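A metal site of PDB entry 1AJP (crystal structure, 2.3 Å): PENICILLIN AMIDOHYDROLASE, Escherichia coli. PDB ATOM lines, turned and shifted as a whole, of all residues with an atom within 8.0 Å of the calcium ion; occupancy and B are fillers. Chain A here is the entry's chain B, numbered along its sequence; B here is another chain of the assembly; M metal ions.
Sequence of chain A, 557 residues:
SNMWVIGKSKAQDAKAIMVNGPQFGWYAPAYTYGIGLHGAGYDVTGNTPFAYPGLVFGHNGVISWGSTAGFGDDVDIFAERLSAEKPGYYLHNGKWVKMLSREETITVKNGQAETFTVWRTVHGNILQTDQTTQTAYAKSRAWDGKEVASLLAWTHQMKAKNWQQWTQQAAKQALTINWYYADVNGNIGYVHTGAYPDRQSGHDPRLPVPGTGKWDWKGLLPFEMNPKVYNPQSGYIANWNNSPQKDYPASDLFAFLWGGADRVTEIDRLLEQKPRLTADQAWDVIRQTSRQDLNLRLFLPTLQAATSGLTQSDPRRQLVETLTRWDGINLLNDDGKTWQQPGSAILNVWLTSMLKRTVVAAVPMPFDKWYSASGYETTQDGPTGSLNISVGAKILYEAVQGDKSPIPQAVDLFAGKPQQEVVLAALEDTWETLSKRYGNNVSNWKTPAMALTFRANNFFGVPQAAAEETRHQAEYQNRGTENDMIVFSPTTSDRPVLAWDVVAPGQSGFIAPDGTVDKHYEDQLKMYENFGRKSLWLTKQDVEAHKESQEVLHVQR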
ATOM      1  N   GLY A  72      13.204 -28.687 -11.763  1.00  0.00           N
ATOM      2  CA  GLY A  72      13.216 -28.817 -13.231  1.00  0.00           C
ATOM      3  C   GLY A  72      13.016 -27.424 -13.792  1.00  0.00           C
ATOM      4  O   GLY A  72      12.675 -26.519 -13.009  1.00  0.00           O
ATOM      5  N   ASP A  73      13.172 -27.209 -15.084  1.00  0.00           N
ATOM      6  CA  ASP A  73      12.918 -25.865 -15.627  1.00  0.00           C
ATOM      7  C   ASP A  73      11.428 -25.829 -16.083  1.00  0.00           C
ATOM      8  O   ASP A  73      11.008 -26.328 -17.138  1.00  0.00           O
ATOM      9  CB  ASP A  73      13.866 -25.462 -16.753  1.00  0.00           C
ATOM     10  CG  ASP A  73      13.614 -24.095 -17.318  1.00  0.00           C
ATOM     11  OD1 ASP A  73      12.595 -23.462 -16.942  1.00  0.00           O
ATOM     12  OD2 ASP A  73      14.276 -23.415 -18.150  1.00  0.00           O
ATOM     13  N   ASP A  74      10.578 -25.173 -15.293  1.00  0.00           N
ATOM     14  CA  ASP A  74       9.160 -25.137 -15.672  1.00  0.00           C
ATOM     15  C   ASP A  74       8.671 -23.715 -15.767  1.00  0.00           C
ATOM     16  O   ASP A  74       7.473 -23.460 -15.678  1.00  0.00           O
ATOM     17  CB  ASP A  74       8.317 -25.973 -14.711  1.00  0.00           C
ATOM     18  CG  ASP A  74       8.457 -25.489 -13.287  1.00  0.00           C
ATOM     19  OD1 ASP A  74       9.167 -24.509 -13.005  1.00  0.00           O
ATOM     20  OD2 ASP A  74       7.895 -25.991 -12.323  1.00  0.00           O
ATOM     21  N   VAL A  75       9.595 -22.769 -15.843  1.00  0.00           N
ATOM     22  CA  VAL A  75       9.235 -21.369 -15.933  1.00  0.00           C
ATOM     23  C   VAL A  75      10.072 -20.729 -17.036  1.00  0.00           C
ATOM     24  O   VAL A  75      11.284 -20.736 -16.815  1.00  0.00           O
ATOM     25  CB  VAL A  75       9.533 -20.689 -14.590  1.00  0.00           C
ATOM     26  CG1 VAL A  75       9.477 -19.179 -14.691  1.00  0.00           C
ATOM     27  CG2 VAL A  75       8.602 -21.084 -13.451  1.00  0.00           C
ATOM     28  N   ASP A  76       9.516 -20.070 -18.044  1.00  0.00           N
ATOM     29  CA  ASP A  76      10.223 -19.301 -19.042  1.00  0.00           C
ATOM     30  C   ASP A  76       9.694 -17.868 -19.080  1.00  0.00           C
ATOM     31  O   ASP A  76       8.542 -17.521 -18.747  1.00  0.00           O
ATOM     32  CB  ASP A  76      10.223 -19.881 -20.473  1.00  0.00           C
ATOM     33  CG  ASP A  76      10.757 -21.268 -20.614  1.00  0.00           C
ATOM     34  OD1 ASP A  76      11.647 -21.714 -19.833  1.00  0.00           O
ATOM     35  OD2 ASP A  76      10.356 -22.055 -21.518  1.00  0.00           O
ATOM     36  N   ILE A  77      10.468 -16.934 -19.604  1.00  0.00           N
ATOM     37  CA  ILE A  77      10.165 -15.517 -19.639  1.00  0.00           C
ATOM     38  C   ILE A  77       9.863 -15.038 -21.057  1.00  0.00           C
ATOM     39  O   ILE A  77      10.592 -15.267 -22.022  1.00  0.00           O
ATOM     40  CB  ILE A  77      11.302 -14.649 -19.073  1.00  0.00           C
ATOM     41  CG1 ILE A  77      11.697 -14.943 -17.628  1.00  0.00           C
ATOM     42  CG2 ILE A  77      10.967 -13.151 -19.223  1.00  0.00           C
ATOM     43  CD1 ILE A  77      10.660 -14.641 -16.581  1.00  0.00           C
ATOM     44  N   SER A 140       6.018 -16.917 -17.457  1.00  0.00           N
ATOM     45  CA  SER A 140       5.082 -17.975 -17.788  1.00  0.00           C
ATOM     46  C   SER A 140       5.452 -19.305 -17.149  1.00  0.00           C
ATOM     47  O   SER A 140       6.576 -19.790 -17.264  1.00  0.00           O
ATOM     48  CB  SER A 140       4.956 -17.929 -19.309  1.00  0.00           C
ATOM     49  OG  SER A 140       4.549 -19.177 -19.787  1.00  0.00           O
ATOM     50  N   PRO A 197       6.835 -27.609 -20.176  1.00  0.00           N
ATOM     51  CA  PRO A 197       6.505 -27.098 -21.488  1.00  0.00           C
ATOM     52  C   PRO A 197       6.998 -27.909 -22.667  1.00  0.00           C
ATOM     53  O   PRO A 197       7.980 -28.621 -22.566  1.00  0.00           O
ATOM     54  CB  PRO A 197       7.058 -25.654 -21.587  1.00  0.00           C
ATOM     55  CG  PRO A 197       8.112 -25.669 -20.499  1.00  0.00           C
ATOM     56  CD  PRO A 197       7.748 -26.701 -19.457  1.00  0.00           C
ATOM     57  N   ARG A 199       8.534 -27.224 -25.840  1.00  0.00           N
ATOM     58  CA  ARG A 199       9.050 -26.008 -26.461  1.00  0.00           C
ATOM     59  C   ARG A 199       9.309 -26.193 -27.946  1.00  0.00           C
ATOM     60  O   ARG A 199       9.519 -27.269 -28.452  1.00  0.00           O
ATOM     61  CB  ARG A 199      10.297 -25.583 -25.697  1.00  0.00           C
ATOM     62  CG  ARG A 199      10.046 -25.195 -24.240  1.00  0.00           C
ATOM     63  CD  ARG A 199      11.335 -24.743 -23.570  1.00  0.00           C
ATOM     64  NE  ARG A 199      11.294 -24.265 -22.199  1.00  0.00           N
ATOM     65  CZ  ARG A 199      11.508 -25.093 -21.163  1.00  0.00           C
ATOM     66  NH1 ARG A 199      11.738 -26.380 -21.293  1.00  0.00           N
ATOM     67  NH2 ARG A 199      11.465 -24.523 -19.979  1.00  0.00           N
ATOM     68  N   HIS A 203      14.503 -23.186 -29.111  1.00  0.00           N
ATOM     69  CA  HIS A 203      14.260 -22.390 -27.916  1.00  0.00           C
ATOM     70  C   HIS A 203      15.321 -22.770 -26.866  1.00  0.00           C
ATOM     71  O   HIS A 203      15.361 -23.911 -26.431  1.00  0.00           O
ATOM     72  CB  HIS A 203      12.847 -22.705 -27.399  1.00  0.00           C
ATOM     73  CG  HIS A 203      12.429 -21.981 -26.154  1.00  0.00           C
ATOM     74  ND1 HIS A 203      11.085 -21.733 -25.870  1.00  0.00           N
ATOM     75  CD2 HIS A 203      13.096 -21.429 -25.113  1.00  0.00           C
ATOM     76  CE1 HIS A 203      10.935 -21.090 -24.750  1.00  0.00           C
ATOM     77  NE2 HIS A 203      12.159 -20.891 -24.268  1.00  0.00           N
ATOM     78  N   ASP A 204      16.174 -21.865 -26.464  1.00  0.00           N
ATOM     79  CA  ASP A 204      17.172 -22.214 -25.406  1.00  0.00           C
ATOM     80  C   ASP A 204      16.490 -21.797 -24.095  1.00  0.00           C
ATOM     81  O   ASP A 204      16.189 -20.603 -23.882  1.00  0.00           O
ATOM     82  CB  ASP A 204      18.425 -21.402 -25.682  1.00  0.00           C
ATOM     83  CG  ASP A 204      19.515 -21.474 -24.622  1.00  0.00           C
ATOM     84  OD1 ASP A 204      19.319 -21.750 -23.398  1.00  0.00           O
ATOM     85  OD2 ASP A 204      20.647 -21.230 -25.088  1.00  0.00           O
ATOM     86  N   PRO A 205      16.136 -22.720 -23.248  1.00  0.00           N
ATOM     87  CA  PRO A 205      15.333 -22.459 -22.078  1.00  0.00           C
ATOM     88  C   PRO A 205      16.018 -21.634 -21.033  1.00  0.00           C
ATOM     89  O   PRO A 205      15.383 -21.386 -20.008  1.00  0.00           O
ATOM     90  CB  PRO A 205      14.844 -23.840 -21.573  1.00  0.00           C
ATOM     91  CG  PRO A 205      15.983 -24.696 -22.065  1.00  0.00           C
ATOM     92  CD  PRO A 205      16.436 -24.161 -23.410  1.00  0.00           C
ATOM     93  N   ARG A 206      17.259 -21.142 -21.185  1.00  0.00           N
ATOM     94  CA  ARG A 206      17.955 -20.431 -20.114  1.00  0.00           C
ATOM     95  C   ARG A 206      17.837 -18.945 -20.276  1.00  0.00           C
ATOM     96  O   ARG A 206      18.303 -18.185 -19.443  1.00  0.00           O
ATOM     97  CB  ARG A 206      19.464 -20.717 -20.075  1.00  0.00           C
ATOM     98  CG  ARG A 206      19.835 -22.195 -19.905  1.00  0.00           C
ATOM     99  CD  ARG A 206      21.239 -22.515 -20.379  1.00  0.00           C
ATOM    100  NE  ARG A 206      21.526 -22.263 -21.781  1.00  0.00           N
ATOM    101  CZ  ARG A 206      22.678 -22.533 -22.407  1.00  0.00           C
ATOM    102  NH1 ARG A 206      23.685 -23.037 -21.684  1.00  0.00           N
ATOM    103  NH2 ARG A 206      22.837 -22.278 -23.708  1.00  0.00           N
ATOM    104  N   LEU A 207      17.268 -18.551 -21.402  1.00  0.00           N
ATOM    105  CA  LEU A 207      17.194 -17.146 -21.810  1.00  0.00           C
ATOM    106  C   LEU A 207      15.803 -16.783 -22.329  1.00  0.00           C
ATOM    107  O   LEU A 207      15.132 -17.587 -22.958  1.00  0.00           O
ATOM    108  CB  LEU A 207      18.200 -16.932 -22.973  1.00  0.00           C
ATOM    109  CG  LEU A 207      19.693 -17.151 -22.646  1.00  0.00           C
ATOM    110  CD1 LEU A 207      20.546 -17.446 -23.858  1.00  0.00           C
ATOM    111  CD2 LEU A 207      20.250 -15.945 -21.922  1.00  0.00           C
ATOM    112  N   PRO A 208      15.462 -15.540 -22.315  1.00  0.00           N
ATOM    113  CA  PRO A 208      14.157 -15.042 -22.741  1.00  0.00           C
ATOM    114  C   PRO A 208      13.747 -15.315 -24.173  1.00  0.00           C
ATOM    115  O   PRO A 208      14.595 -15.506 -25.049  1.00  0.00           O
ATOM    116  CB  PRO A 208      14.133 -13.519 -22.475  1.00  0.00           C
ATOM    117  CG  PRO A 208      15.168 -13.396 -21.385  1.00  0.00           C
ATOM    118  CD  PRO A 208      16.197 -14.503 -21.582  1.00  0.00           C
ATOM    119  N   TRP A 217       4.973 -21.857 -26.412  1.00  0.00           N
ATOM    120  CA  TRP A 217       5.036 -23.281 -26.173  1.00  0.00           C
ATOM    121  C   TRP A 217       3.942 -23.948 -27.024  1.00  0.00           C
ATOM    122  O   TRP A 217       2.905 -23.362 -27.318  1.00  0.00           O
ATOM    123  CB  TRP A 217       4.768 -23.634 -24.718  1.00  0.00           C
ATOM    124  CG  TRP A 217       5.688 -23.017 -23.706  1.00  0.00           C
ATOM    125  CD1 TRP A 217       6.978 -22.617 -23.891  1.00  0.00           C
ATOM    126  CD2 TRP A 217       5.393 -22.831 -22.319  1.00  0.00           C
ATOM    127  NE1 TRP A 217       7.458 -22.100 -22.724  1.00  0.00           N
ATOM    128  CE2 TRP A 217       6.538 -22.250 -21.728  1.00  0.00           C
ATOM    129  CE3 TRP A 217       4.258 -23.041 -21.528  1.00  0.00           C
ATOM    130  CZ2 TRP A 217       6.618 -21.917 -20.383  1.00  0.00           C
ATOM    131  CZ3 TRP A 217       4.347 -22.696 -20.183  1.00  0.00           C
ATOM    132  CH2 TRP A 217       5.497 -22.162 -19.613  1.00  0.00           C
ATOM    133  N   ALA A 250      18.244 -28.872 -15.751  1.00  0.00           N
ATOM    134  CA  ALA A 250      17.888 -28.294 -14.482  1.00  0.00           C
ATOM    135  C   ALA A 250      17.275 -26.900 -14.700  1.00  0.00           C
ATOM    136  O   ALA A 250      17.341 -26.267 -15.764  1.00  0.00           O
ATOM    137  CB  ALA A 250      19.186 -28.035 -13.714  1.00  0.00           C
ATOM    138  N   SER A 251      16.726 -26.385 -13.616  1.00  0.00           N
ATOM    139  CA  SER A 251      16.186 -25.046 -13.515  1.00  0.00           C
ATOM    140  C   SER A 251      17.139 -24.128 -14.277  1.00  0.00           C
ATOM    141  O   SER A 251      18.345 -24.352 -14.134  1.00  0.00           O
ATOM    142  CB  SER A 251      16.335 -24.642 -12.040  1.00  0.00           C
ATOM    143  OG  SER A 251      15.965 -23.314 -11.865  1.00  0.00           O
ATOM    144  N   ASP A 252      16.709 -22.988 -14.767  1.00  0.00           N
ATOM    145  CA  ASP A 252      17.556 -22.015 -15.429  1.00  0.00           C
ATOM    146  C   ASP A 252      18.239 -21.042 -14.459  1.00  0.00           C
ATOM    147  O   ASP A 252      18.994 -20.196 -14.966  1.00  0.00           O
ATOM    148  CB  ASP A 252      16.831 -21.230 -16.529  1.00  0.00           C
ATOM    149  CG  ASP A 252      15.698 -20.366 -15.988  1.00  0.00           C
ATOM    150  OD1 ASP A 252      15.935 -19.557 -15.038  1.00  0.00           O
ATOM    151  OD2 ASP A 252      14.553 -20.476 -16.539  1.00  0.00           O
ATOM    152  N   LEU A 253      18.062 -21.175 -13.141  1.00  0.00           N
ATOM    153  CA  LEU A 253      18.794 -20.311 -12.218  1.00  0.00           C
ATOM    154  C   LEU A 253      20.342 -20.309 -12.466  1.00  0.00           C
ATOM    155  O   LEU A 253      20.949 -21.393 -12.471  1.00  0.00           O
ATOM    156  CB  LEU A 253      18.658 -20.756 -10.756  1.00  0.00           C
ATOM    157  CG  LEU A 253      17.291 -20.528 -10.159  1.00  0.00           C
ATOM    158  CD1 LEU A 253      17.099 -21.288  -8.862  1.00  0.00           C
ATOM    159  CD2 LEU A 253      17.112 -19.027  -9.960  1.00  0.00           C
ATOM    160  N   SER B 149      11.130 -20.787  -9.811  1.00  0.00           N
ATOM    161  CA  SER B 149      12.475 -20.205  -9.855  1.00  0.00           C
ATOM    162  C   SER B 149      12.883 -19.854 -11.271  1.00  0.00           C
ATOM    163  O   SER B 149      12.802 -20.828 -12.056  1.00  0.00           O
ATOM    164  CB  SER B 149      13.406 -21.318  -9.385  1.00  0.00           C
ATOM    165  OG  SER B 149      13.403 -21.457  -8.000  1.00  0.00           O
ATOM    166  N   THR B 150      13.313 -18.643 -11.584  1.00  0.00           N
ATOM    167  CA  THR B 150      13.843 -18.416 -12.928  1.00  0.00           C
ATOM    168  C   THR B 150      14.877 -17.278 -12.786  1.00  0.00           C
ATOM    169  O   THR B 150      14.617 -16.453 -11.917  1.00  0.00           O
ATOM    170  CB  THR B 150      12.818 -18.016 -13.987  1.00  0.00           C
ATOM    171  OG1 THR B 150      13.414 -17.930 -15.313  1.00  0.00           O
ATOM    172  CG2 THR B 150      12.268 -16.599 -13.762  1.00  0.00           C
ATOM    173  N   SER B 151      15.857 -17.126 -13.670  1.00  0.00           N
ATOM    174  CA  SER B 151      16.764 -15.945 -13.583  1.00  0.00           C
ATOM    175  C   SER B 151      17.059 -15.567 -15.047  1.00  0.00           C
ATOM    176  O   SER B 151      18.060 -14.913 -15.312  1.00  0.00           O
ATOM    177  CB  SER B 151      18.071 -16.159 -12.813  1.00  0.00           C
ATOM    178  OG  SER B 151      18.925 -17.167 -13.385  1.00  0.00           O
ATOM    179  N   GLU B 152      16.094 -15.824 -15.950  1.00  0.00           N
ATOM    180  CA  GLU B 152      16.314 -15.715 -17.360  1.00  0.00           C
ATOM    181  C   GLU B 152      16.776 -14.320 -17.773  1.00  0.00           C
ATOM    182  O   GLU B 152      17.669 -14.138 -18.635  1.00  0.00           O
ATOM    183  CB  GLU B 152      15.229 -16.200 -18.309  1.00  0.00           C
ATOM    184  CG  GLU B 152      15.048 -17.711 -18.380  1.00  0.00           C
ATOM    185  CD  GLU B 152      13.847 -18.118 -19.230  1.00  0.00           C
ATOM    186  OE1 GLU B 152      13.402 -17.207 -19.987  1.00  0.00           O
ATOM    187  OE2 GLU B 152      13.398 -19.303 -19.150  1.00  0.00           O
ATOM    188  N   ASN B 155      20.316 -13.988 -16.627  1.00  0.00           N
ATOM    189  CA  ASN B 155      21.170 -14.751 -17.498  1.00  0.00           C
ATOM    190  C   ASN B 155      21.544 -13.928 -18.752  1.00  0.00           C
ATOM    191  O   ASN B 155      22.707 -13.918 -19.183  1.00  0.00           O
ATOM    192  CB  ASN B 155      20.624 -16.090 -17.899  1.00  0.00           C
ATOM    193  CG  ASN B 155      20.355 -16.991 -16.694  1.00  0.00           C
ATOM    194  OD1 ASN B 155      20.653 -16.556 -15.597  1.00  0.00           O
ATOM    195  ND2 ASN B 155      19.732 -18.133 -16.951  1.00  0.00           N
HETATM  196 CA    CA M   1      13.397 -21.317 -18.316  1.00  0.00          CA
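N of Glu 152 of chain B is in hydrogen-bond range of OG1 of Thr 150 of chain B (3.5 Å).
The backbone NH of Ile 77 is in hydrogen-bond range of the side-chain carboxylate of Glu 152 of chain B, 3.0 Å away.
The side-chain carboxylate of Asp 252 lies within hydrogen-bond range of the side-chain hydroxyl of Thr 150 of chain B, at 3.0 Å.
The backbone carbonyl oxygen of Asp 252 lies within hydrogen-bond range of the side-chain amide nitrogen of Asn 155 of chain B, 3.0 Å away.
OD2 of Asp 76 lies within salt-bridge range of NE of Arg 199.
OD2 of Asp 76 sits close to NE2 of His 203 (3.5 Å).
The backbone carbonyl oxygen of Asp 76 is in hydrogen-bond range of the backbone NH of Ser 140.
NE1 of Trp 217 sits at hydrogen-bond distance from OD2 of Asp 76, at 3.1 Å.
The calcium ion is bound by OE2 of Glu 152 of chain B (2.2 Å), OD2 of Asp 252 (2.3 Å), OD2 of Asp 73 (2.3 Å), OD1 of Asp 76 (2.3 Å), O of Pro 205 (2.6 Å), O of Val 75 (2.7 Å) and OD1 of Asp 73 (2.7 Å).
The calcium ion has seven donor atoms within binding distance.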
